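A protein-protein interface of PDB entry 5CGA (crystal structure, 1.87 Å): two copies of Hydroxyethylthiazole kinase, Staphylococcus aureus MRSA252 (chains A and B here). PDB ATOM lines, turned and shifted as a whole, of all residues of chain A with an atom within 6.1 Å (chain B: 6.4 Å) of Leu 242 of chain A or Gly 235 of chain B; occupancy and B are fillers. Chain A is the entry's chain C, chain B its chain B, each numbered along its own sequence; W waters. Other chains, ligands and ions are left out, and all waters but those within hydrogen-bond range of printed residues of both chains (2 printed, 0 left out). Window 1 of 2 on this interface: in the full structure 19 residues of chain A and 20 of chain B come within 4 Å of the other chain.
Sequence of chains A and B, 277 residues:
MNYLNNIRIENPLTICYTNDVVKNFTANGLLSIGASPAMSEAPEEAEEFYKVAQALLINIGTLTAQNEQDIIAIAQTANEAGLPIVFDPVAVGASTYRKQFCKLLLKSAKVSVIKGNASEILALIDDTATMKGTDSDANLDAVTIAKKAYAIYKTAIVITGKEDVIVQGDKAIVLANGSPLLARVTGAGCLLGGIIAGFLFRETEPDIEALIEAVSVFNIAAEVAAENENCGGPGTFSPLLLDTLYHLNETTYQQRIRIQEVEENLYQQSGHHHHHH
OG1 of Thr 236 of chain B sits at hydrogen-bond distance from N of Gly 232 of chain B (2.7 Å).
The side-chain hydroxyl of Thr 236 of chain B sits at hydrogen-bond distance from the backbone NH of Gly 233 of chain B, 3.4 Å away.
OG of Ser 32 of chain A is in hydrogen-bond range of O of Gly 29 of chain A, at 2.8 Å.
The side-chain hydroxyl (OG1) of Thr 244 of chain A is in hydrogen-bond range of the backbone carbonyl oxygen (O) of Leu 240 of chain A (2.8 Å).
OD1 of Asn 28 of chain A touches O of Arg 184 of chain B (3.9 Å).
Asn 28 of chain A touches Val 185 of chain B (OD1 to C, 3.6 Å).
O of Pro 239 of chain A touches CA of Gly 235 of chain B, at 3.4 Å.
Pro 239 of chain A touches Thr 236 of chain B.
Leu 240 of chain A touches Thr 236 of chain B.
CA of Gly 235 of chain B touches CB of Leu 242 of chain A, at 3.7 Å.
C of Gly 232 of chain B touches OD2 of Asp 243 of chain A (3.4 Å).
CE1 of Tyr 246 of chain A touches NH1 of Arg 184 of chain B (3.7 Å).
Tyr 246 of chain A touches Pro 234 of chain B (CG to CD, 3.3 Å).
Of the printed residues of chain B, Ser 32 of chain A touches Arg 184.
Ser 238 of chain A touches none of the printed residues of chain B.
Of chain B, only Gly 235 (3.7 Å) comes within 4 Å of Leu 242 of chain A.
Of the printed residues of chain A, Val 185 of chain B touches Asn 28 (3.6 Å).
Of the printed residues of chain A, Gly 233 of chain B touches Asp 243.
Of the printed residues of chain A, Pro 234 of chain B touches Asp 243 (3.4 Å) and Tyr 246 (3.3 Å).
Gly 235 of chain B touches three residues of chain A.
The nearest residue of chain A that does not touch Gly 235 of chain B is Leu 240 of chain A (5.3 Å).
The nearest printed residue of chain A that does not touch Arg 184 of chain B is Leu 30 of chain A (5.9 Å).
O of Ser 32 of chain A sits at hydrogen-bond distance from NH2 of Arg 184 of chain B.
O of Gly 232 of chain B sits at hydrogen-bond distance from NE2 of His 247 of chain A, at 2.7 Å.
OD1 of Asp 243 of chain A sits close to N of Gly 233 of chain B (3.4 Å).
The side-chain carboxylate of Asp 243 of chain A lies within hydrogen-bond range of the backbone NH of Gly 235 of chain B, at 2.8 Å.
The side-chain hydroxyl (OG1) of Thr 236 of chain B sits at hydrogen-bond distance from the side-chain carboxylate (OD2) of Asp 243 of chain A (2.6 Å).
OD1 of Asp 243 of chain A lies close to N of Pro 234 of chain B.
Positions printed for both chains: 237, 238, 239 and 240.
Of the 15 pairs that touch across the chains among the printed residues, none has its exchanged pair printed and touching as well.
Of the 18 printed residues of chain A, 8 touch a printed residue of chain B.
Hydrophobic or aromatic side chains of chain A that line the printed part of chain B: Pro 239, Leu 240, Leu 242, Tyr 246 and His 247.
Hydrophobic or aromatic side chains of chain B that line the printed part of chain A: Pro 234.
Among the printed residues, no Asp or Glu carboxylate lies within 4 Å of a Lys or Arg side-chain nitrogen of the other chain.
Water W1 lies within hydrogen-bond range of O of Arg 184 of chain B and O of Asn 28 of chain A.
Water W2 lies within hydrogen-bond range of O of Gly 232 of chain B and NE2 of His 247 of chain A.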
ATOM      1  N   PHE A  25     -15.975  21.883  10.920  1.00  0.00           N
ATOM      2  CA  PHE A  25     -15.840  21.026   9.763  1.00  0.00           C
ATOM      3  C   PHE A  25     -15.316  19.698  10.155  1.00  0.00           C
ATOM      4  O   PHE A  25     -15.784  18.665   9.663  1.00  0.00           O
ATOM      5  CB  PHE A  25     -14.929  21.714   8.749  1.00  0.00           C
ATOM      6  CG  PHE A  25     -14.805  21.029   7.459  1.00  0.00           C
ATOM      7  CD1 PHE A  25     -15.886  20.653   6.720  1.00  0.00           C
ATOM      8  CD2 PHE A  25     -13.542  20.860   6.906  1.00  0.00           C
ATOM      9  CE1 PHE A  25     -15.784  20.007   5.483  1.00  0.00           C
ATOM     10  CE2 PHE A  25     -13.437  20.260   5.648  1.00  0.00           C
ATOM     11  CZ  PHE A  25     -14.571  19.848   4.948  1.00  0.00           C
ATOM     12  N   ASN A  28     -18.237  17.820  11.754  1.00  0.00           N
ATOM     13  CA  ASN A  28     -19.159  17.364  10.714  1.00  0.00           C
ATOM     14  C   ASN A  28     -18.654  16.238   9.841  1.00  0.00           C
ATOM     15  O   ASN A  28     -19.416  15.352   9.496  1.00  0.00           O
ATOM     16  CB  ASN A  28     -19.624  18.523   9.837  1.00  0.00           C
ATOM     17  CG  ASN A  28     -20.701  19.339  10.513  1.00  0.00           C
ATOM     18  OD1 ASN A  28     -21.541  18.805  11.183  1.00  0.00           O
ATOM     19  ND2 ASN A  28     -20.595  20.614  10.450  1.00  0.00           N
ATOM     20  N   GLY A  29     -17.383  16.254   9.521  1.00  0.00           N
ATOM     21  CA  GLY A  29     -16.767  15.154   8.751  1.00  0.00           C
ATOM     22  C   GLY A  29     -16.821  13.849   9.534  1.00  0.00           C
ATOM     23  O   GLY A  29     -17.172  12.810   9.012  1.00  0.00           O
ATOM     24  N   LEU A  30     -16.480  13.909  10.838  1.00  0.00           N
ATOM     25  CA  LEU A  30     -16.602  12.762  11.752  1.00  0.00           C
ATOM     26  C   LEU A  30     -18.011  12.262  11.909  1.00  0.00           C
ATOM     27  O   LEU A  30     -18.286  11.067  11.782  1.00  0.00           O
ATOM     28  CB  LEU A  30     -15.986  13.053  13.087  1.00  0.00           C
ATOM     29  CG  LEU A  30     -14.447  12.949  13.086  1.00  0.00           C
ATOM     30  CD1 LEU A  30     -13.862  13.622  14.284  1.00  0.00           C
ATOM     31  CD2 LEU A  30     -14.043  11.488  13.034  1.00  0.00           C
ATOM     32  N   SER A  32     -20.303  12.545   9.581  1.00  0.00           N
ATOM     33  CA  SER A  32     -20.729  12.029   8.346  1.00  0.00           C
ATOM     34  C   SER A  32     -20.298  10.590   8.117  1.00  0.00           C
ATOM     35  O   SER A  32     -21.068   9.825   7.526  1.00  0.00           O
ATOM     36  CB  SER A  32     -20.396  12.968   7.184  1.00  0.00           C
ATOM     37  OG  SER A  32     -19.011  12.684   6.844  1.00  0.00           O
ATOM     38  N   LEU A 191      -9.337  18.016   8.793  1.00  0.00           N
ATOM     39  CA  LEU A 191     -10.396  17.059   8.940  1.00  0.00           C
ATOM     40  C   LEU A 191      -9.790  15.629   8.735  1.00  0.00           C
ATOM     41  O   LEU A 191     -10.251  14.682   9.342  1.00  0.00           O
ATOM     42  CB  LEU A 191     -11.536  17.291   7.920  1.00  0.00           C
ATOM     43  CG  LEU A 191     -12.492  16.192   7.697  1.00  0.00           C
ATOM     44  CD1 LEU A 191     -13.213  15.722   8.977  1.00  0.00           C
ATOM     45  CD2 LEU A 191     -13.544  16.675   6.687  1.00  0.00           C
ATOM     46  N   ALA A 225     -17.224  13.541  -4.836  1.00  0.00           N
ATOM     47  CA  ALA A 225     -17.905  14.849  -4.615  1.00  0.00           C
ATOM     48  C   ALA A 225     -17.592  15.825  -5.757  1.00  0.00           C
ATOM     49  O   ALA A 225     -18.469  16.572  -6.247  1.00  0.00           O
ATOM     50  CB  ALA A 225     -17.543  15.424  -3.293  1.00  0.00           C
ATOM     51  N   PHE A 237     -18.502  22.376  -3.005  1.00  0.00           N
ATOM     52  CA  PHE A 237     -17.755  21.095  -2.776  1.00  0.00           C
ATOM     53  C   PHE A 237     -17.796  20.561  -1.358  1.00  0.00           C
ATOM     54  O   PHE A 237     -18.037  19.365  -1.153  1.00  0.00           O
ATOM     55  CB  PHE A 237     -16.335  21.262  -3.247  1.00  0.00           C
ATOM     56  CG  PHE A 237     -15.453  20.085  -2.883  1.00  0.00           C
ATOM     57  CD1 PHE A 237     -15.465  18.940  -3.656  1.00  0.00           C
ATOM     58  CD2 PHE A 237     -14.630  20.171  -1.832  1.00  0.00           C
ATOM     59  CE1 PHE A 237     -14.583  17.905  -3.361  1.00  0.00           C
ATOM     60  CE2 PHE A 237     -13.845  19.095  -1.437  1.00  0.00           C
ATOM     61  CZ  PHE A 237     -13.761  18.007  -2.287  1.00  0.00           C
ATOM     62  N   SER A 238     -17.742  21.422  -0.374  1.00  0.00           N
ATOM     63  CA  SER A 238     -17.658  21.023   1.006  1.00  0.00           C
ATOM     64  C   SER A 238     -18.890  20.313   1.562  1.00  0.00           C
ATOM     65  O   SER A 238     -18.781  19.190   2.023  1.00  0.00           O
ATOM     66  CB  SER A 238     -17.233  22.204   1.836  1.00  0.00           C
ATOM     67  OG  SER A 238     -17.329  21.860   3.174  1.00  0.00           O
ATOM     68  N   PRO A 239     -20.105  20.822   1.275  1.00  0.00           N
ATOM     69  CA  PRO A 239     -21.273  20.046   1.560  1.00  0.00           C
ATOM     70  C   PRO A 239     -21.356  18.754   0.823  1.00  0.00           C
ATOM     71  O   PRO A 239     -21.802  17.696   1.385  1.00  0.00           O
ATOM     72  CB  PRO A 239     -22.452  21.007   1.157  1.00  0.00           C
ATOM     73  CG  PRO A 239     -21.835  22.359   1.378  1.00  0.00           C
ATOM     74  CD  PRO A 239     -20.417  22.226   0.922  1.00  0.00           C
ATOM     75  N   LEU A 240     -20.966  18.734  -0.428  1.00  0.00           N
ATOM     76  CA  LEU A 240     -20.987  17.516  -1.230  1.00  0.00           C
ATOM     77  C   LEU A 240     -20.002  16.456  -0.648  1.00  0.00           C
ATOM     78  O   LEU A 240     -20.293  15.251  -0.758  1.00  0.00           O
ATOM     79  CB  LEU A 240     -20.784  17.843  -2.688  1.00  0.00           C
ATOM     80  CG  LEU A 240     -21.916  18.619  -3.336  1.00  0.00           C
ATOM     81  CD1 LEU A 240     -21.502  19.105  -4.689  1.00  0.00           C
ATOM     82  CD2 LEU A 240     -23.165  17.827  -3.454  1.00  0.00           C
ATOM     83  N   LEU A 241     -18.862  16.882  -0.201  1.00  0.00           N
ATOM     84  CA  LEU A 241     -17.872  15.984   0.398  1.00  0.00           C
ATOM     85  C   LEU A 241     -18.474  15.279   1.592  1.00  0.00           C
ATOM     86  O   LEU A 241     -18.393  14.055   1.740  1.00  0.00           O
ATOM     87  CB  LEU A 241     -16.644  16.788   0.803  1.00  0.00           C
ATOM     88  CG  LEU A 241     -15.613  15.981   1.613  1.00  0.00           C
ATOM     89  CD1 LEU A 241     -15.050  14.854   0.766  1.00  0.00           C
ATOM     90  CD2 LEU A 241     -14.545  16.898   2.054  1.00  0.00           C
ATOM     91  N   LEU A 242     -19.148  16.037   2.421  1.00  0.00           N
ATOM     92  CA  LEU A 242     -19.837  15.423   3.575  1.00  0.00           C
ATOM     93  C   LEU A 242     -20.905  14.454   3.101  1.00  0.00           C
ATOM     94  O   LEU A 242     -21.049  13.399   3.734  1.00  0.00           O
ATOM     95  CB  LEU A 242     -20.345  16.500   4.536  1.00  0.00           C
ATOM     96  CG  LEU A 242     -19.340  17.461   5.097  1.00  0.00           C
ATOM     97  CD1 LEU A 242     -20.005  18.570   5.891  1.00  0.00           C
ATOM     98  CD2 LEU A 242     -18.386  16.777   6.021  1.00  0.00           C
ATOM     99  N   ASP A 243     -21.739  14.794   2.114  1.00  0.00           N
ATOM    100  CA  ASP A 243     -22.741  13.881   1.646  1.00  0.00           C
ATOM    101  C   ASP A 243     -22.094  12.584   1.149  1.00  0.00           C
ATOM    102  O   ASP A 243     -22.586  11.498   1.312  1.00  0.00           O
ATOM    103  CB  ASP A 243     -23.490  14.436   0.472  1.00  0.00           C
ATOM    104  CG  ASP A 243     -24.469  15.558   0.869  1.00  0.00           C
ATOM    105  OD1 ASP A 243     -24.618  15.837   2.089  1.00  0.00           O
ATOM    106  OD2 ASP A 243     -25.110  16.134  -0.117  1.00  0.00           O
ATOM    107  N   THR A 244     -20.994  12.741   0.417  1.00  0.00           N
ATOM    108  CA  THR A 244     -20.286  11.597  -0.205  1.00  0.00           C
ATOM    109  C   THR A 244     -19.653  10.671   0.849  1.00  0.00           C
ATOM    110  O   THR A 244     -19.768   9.456   0.680  1.00  0.00           O
ATOM    111  CB  THR A 244     -19.250  12.130  -1.219  1.00  0.00           C
ATOM    112  OG1 THR A 244     -19.947  12.921  -2.184  1.00  0.00           O
ATOM    113  CG2 THR A 244     -18.684  10.976  -1.949  1.00  0.00           C
ATOM    114  N   LEU A 245     -19.105  11.225   1.903  1.00  0.00           N
ATOM    115  CA  LEU A 245     -18.606  10.467   3.054  1.00  0.00           C
ATOM    116  C   LEU A 245     -19.753   9.695   3.694  1.00  0.00           C
ATOM    117  O   LEU A 245     -19.643   8.534   3.998  1.00  0.00           O
ATOM    118  CB  LEU A 245     -17.993  11.365   4.109  1.00  0.00           C
ATOM    119  CG  LEU A 245     -16.644  11.987   3.759  1.00  0.00           C
ATOM    120  CD1 LEU A 245     -16.212  13.102   4.661  1.00  0.00           C
ATOM    121  CD2 LEU A 245     -15.583  10.858   3.754  1.00  0.00           C
ATOM    122  N   TYR A 246     -20.890  10.359   3.848  1.00  0.00           N
ATOM    123  CA  TYR A 246     -22.078   9.684   4.385  1.00  0.00           C
ATOM    124  C   TYR A 246     -22.573   8.515   3.593  1.00  0.00           C
ATOM    125  O   TYR A 246     -22.978   7.501   4.167  1.00  0.00           O
ATOM    126  CB  TYR A 246     -23.135  10.768   4.578  1.00  0.00           C
ATOM    127  CG  TYR A 246     -24.503  10.323   5.023  1.00  0.00           C
ATOM    128  CD1 TYR A 246     -24.772  10.207   6.361  1.00  0.00           C
ATOM    129  CD2 TYR A 246     -25.475  10.052   4.123  1.00  0.00           C
ATOM    130  CE1 TYR A 246     -26.067   9.856   6.765  1.00  0.00           C
ATOM    131  CE2 TYR A 246     -26.809   9.707   4.519  1.00  0.00           C
ATOM    132  CZ  TYR A 246     -27.029   9.621   5.889  1.00  0.00           C
ATOM    133  OH  TYR A 246     -28.297   9.195   6.262  1.00  0.00           O
ATOM    134  N   HIS A 247     -22.567   8.601   2.252  1.00  0.00           N
ATOM    135  CA  HIS A 247     -23.058   7.621   1.372  1.00  0.00           C
ATOM    136  C   HIS A 247     -22.012   6.588   0.866  1.00  0.00           C
ATOM    137  O   HIS A 247     -22.402   5.650   0.247  1.00  0.00           O
ATOM    138  CB  HIS A 247     -23.722   8.246   0.105  1.00  0.00           C
ATOM    139  CG  HIS A 247     -25.046   8.893   0.354  1.00  0.00           C
ATOM    140  ND1 HIS A 247     -26.153   8.176   0.769  1.00  0.00           N
ATOM    141  CD2 HIS A 247     -25.406  10.216   0.374  1.00  0.00           C
ATOM    142  CE1 HIS A 247     -27.159   9.032   0.993  1.00  0.00           C
ATOM    143  NE2 HIS A 247     -26.721  10.262   0.751  1.00  0.00           N
ATOM    144  N   ARG B 184     -26.785  14.596  12.535  1.00  0.00           N
ATOM    145  CA  ARG B 184     -25.543  14.383  11.740  1.00  0.00           C
ATOM    146  C   ARG B 184     -24.998  15.687  11.312  1.00  0.00           C
ATOM    147  O   ARG B 184     -23.967  15.751  10.624  1.00  0.00           O
ATOM    148  CB  ARG B 184     -25.817  13.466  10.583  1.00  0.00           C
ATOM    149  CG  ARG B 184     -26.510  12.163  10.943  1.00  0.00           C
ATOM    150  CD  ARG B 184     -25.657  11.316  11.870  1.00  0.00           C
ATOM    151  NE  ARG B 184     -24.532  10.736  11.102  1.00  0.00           N
ATOM    152  CZ  ARG B 184     -24.596   9.645  10.376  1.00  0.00           C
ATOM    153  NH1 ARG B 184     -25.754   8.908  10.322  1.00  0.00           N
ATOM    154  NH2 ARG B 184     -23.513   9.206   9.741  1.00  0.00           N
ATOM    155  N   VAL B 185     -25.540  16.735  11.863  1.00  0.00           N
ATOM    156  CA  VAL B 185     -25.036  18.037  11.686  1.00  0.00           C
ATOM    157  C   VAL B 185     -24.604  18.571  13.029  1.00  0.00           C
ATOM    158  O   VAL B 185     -25.388  18.650  13.988  1.00  0.00           O
ATOM    159  CB  VAL B 185     -26.123  18.951  11.109  1.00  0.00           C
ATOM    160  CG1 VAL B 185     -25.592  20.362  11.037  1.00  0.00           C
ATOM    161  CG2 VAL B 185     -26.609  18.415   9.784  1.00  0.00           C
ATOM    162  N   GLY B 232     -28.950  15.834  -0.360  1.00  0.00           N
ATOM    163  CA  GLY B 232     -28.323  14.540  -0.732  1.00  0.00           C
ATOM    164  C   GLY B 232     -27.587  13.900   0.481  1.00  0.00           C
ATOM    165  O   GLY B 232     -26.928  12.889   0.308  1.00  0.00           O
ATOM    166  N   GLY B 233     -27.732  14.447   1.652  1.00  0.00           N
ATOM    167  CA  GLY B 233     -27.078  13.981   2.909  1.00  0.00           C
ATOM    168  C   GLY B 233     -26.843  15.049   3.891  1.00  0.00           C
ATOM    169  O   GLY B 233     -27.366  16.140   3.734  1.00  0.00           O
ATOM    170  N   PRO B 234     -26.073  14.804   4.992  1.00  0.00           N
ATOM    171  CA  PRO B 234     -25.915  15.754   6.056  1.00  0.00           C
ATOM    172  C   PRO B 234     -25.192  17.003   5.665  1.00  0.00           C
ATOM    173  O   PRO B 234     -25.414  18.035   6.239  1.00  0.00           O
ATOM    174  CB  PRO B 234     -25.128  15.009   7.152  1.00  0.00           C
ATOM    175  CG  PRO B 234     -24.480  13.971   6.457  1.00  0.00           C
ATOM    176  CD  PRO B 234     -25.328  13.556   5.256  1.00  0.00           C
ATOM    177  N   GLY B 235     -24.344  16.924   4.639  1.00  0.00           N
ATOM    178  CA  GLY B 235     -23.619  18.121   4.200  1.00  0.00           C
ATOM    179  C   GLY B 235     -24.545  19.112   3.445  1.00  0.00           C
ATOM    180  O   GLY B 235     -24.565  20.266   3.836  1.00  0.00           O
ATOM    181  N   THR B 236     -25.295  18.667   2.483  1.00  0.00           N
ATOM    182  CA  THR B 236     -26.251  19.552   1.777  1.00  0.00           C
ATOM    183  C   THR B 236     -27.458  19.883   2.620  1.00  0.00           C
ATOM    184  O   THR B 236     -28.039  20.985   2.458  1.00  0.00           O
ATOM    185  CB  THR B 236     -26.681  18.983   0.450  1.00  0.00           C
ATOM    186  OG1 THR B 236     -27.080  17.608   0.560  1.00  0.00           O
ATOM    187  CG2 THR B 236     -25.552  19.119  -0.605  1.00  0.00           C
ATOM    188  N   PHE B 237     -27.763  19.040   3.595  1.00  0.00           N
ATOM    189  CA  PHE B 237     -28.854  19.334   4.557  1.00  0.00           C
ATOM    190  C   PHE B 237     -28.695  20.606   5.309  1.00  0.00           C
ATOM    191  O   PHE B 237     -29.631  21.408   5.479  1.00  0.00           O
ATOM    192  CB  PHE B 237     -29.028  18.173   5.503  1.00  0.00           C
ATOM    193  CG  PHE B 237     -29.961  18.449   6.602  1.00  0.00           C
ATOM    194  CD1 PHE B 237     -31.337  18.270   6.388  1.00  0.00           C
ATOM    195  CD2 PHE B 237     -29.514  18.733   7.845  1.00  0.00           C
ATOM    196  CE1 PHE B 237     -32.218  18.493   7.460  1.00  0.00           C
ATOM    197  CE2 PHE B 237     -30.406  18.957   8.928  1.00  0.00           C
ATOM    198  CZ  PHE B 237     -31.753  18.869   8.692  1.00  0.00           C
ATOM    199  N   SER B 238     -27.480  20.944   5.755  1.00  0.00           N
ATOM    200  CA  SER B 238     -27.264  22.104   6.573  1.00  0.00           C
ATOM    201  C   SER B 238     -27.594  23.460   5.913  1.00  0.00           C
ATOM    202  O   SER B 238     -28.382  24.245   6.473  1.00  0.00           O
ATOM    203  CB  SER B 238     -25.860  22.064   7.237  1.00  0.00           C
ATOM    204  OG  SER B 238     -25.642  23.283   7.904  1.00  0.00           O
ATOM    205  N   PRO B 239     -27.074  23.717   4.746  1.00  0.00           N
ATOM    206  CA  PRO B 239     -27.512  24.912   4.003  1.00  0.00           C
ATOM    207  C   PRO B 239     -29.034  24.905   3.704  1.00  0.00           C
ATOM    208  O   PRO B 239     -29.674  25.986   3.862  1.00  0.00           O
ATOM    209  CB  PRO B 239     -26.743  24.855   2.714  1.00  0.00           C
ATOM    210  CG  PRO B 239     -25.458  24.081   3.081  1.00  0.00           C
ATOM    211  CD  PRO B 239     -25.935  23.041   4.087  1.00  0.00           C
ATOM    212  N   LEU B 240     -29.593  23.764   3.399  1.00  0.00           N
ATOM    213  CA  LEU B 240     -31.023  23.663   3.193  1.00  0.00           C
ATOM    214  C   LEU B 240     -31.835  23.978   4.441  1.00  0.00           C
ATOM    215  O   LEU B 240     -32.935  24.574   4.348  1.00  0.00           O
ATOM    216  CB  LEU B 240     -31.441  22.376   2.527  1.00  0.00           C
ATOM    217  CG  LEU B 240     -30.844  22.179   1.108  1.00  0.00           C
ATOM    218  CD1 LEU B 240     -31.098  20.797   0.677  1.00  0.00           C
ATOM    219  CD2 LEU B 240     -31.550  23.107   0.130  1.00  0.00           C
HETATM  220  O   HOH W   1     -22.146  15.948   8.768  1.00  0.00           O
HETATM  221  O   HOH W   2     -26.346  12.118  -2.183  1.00  0.00           O
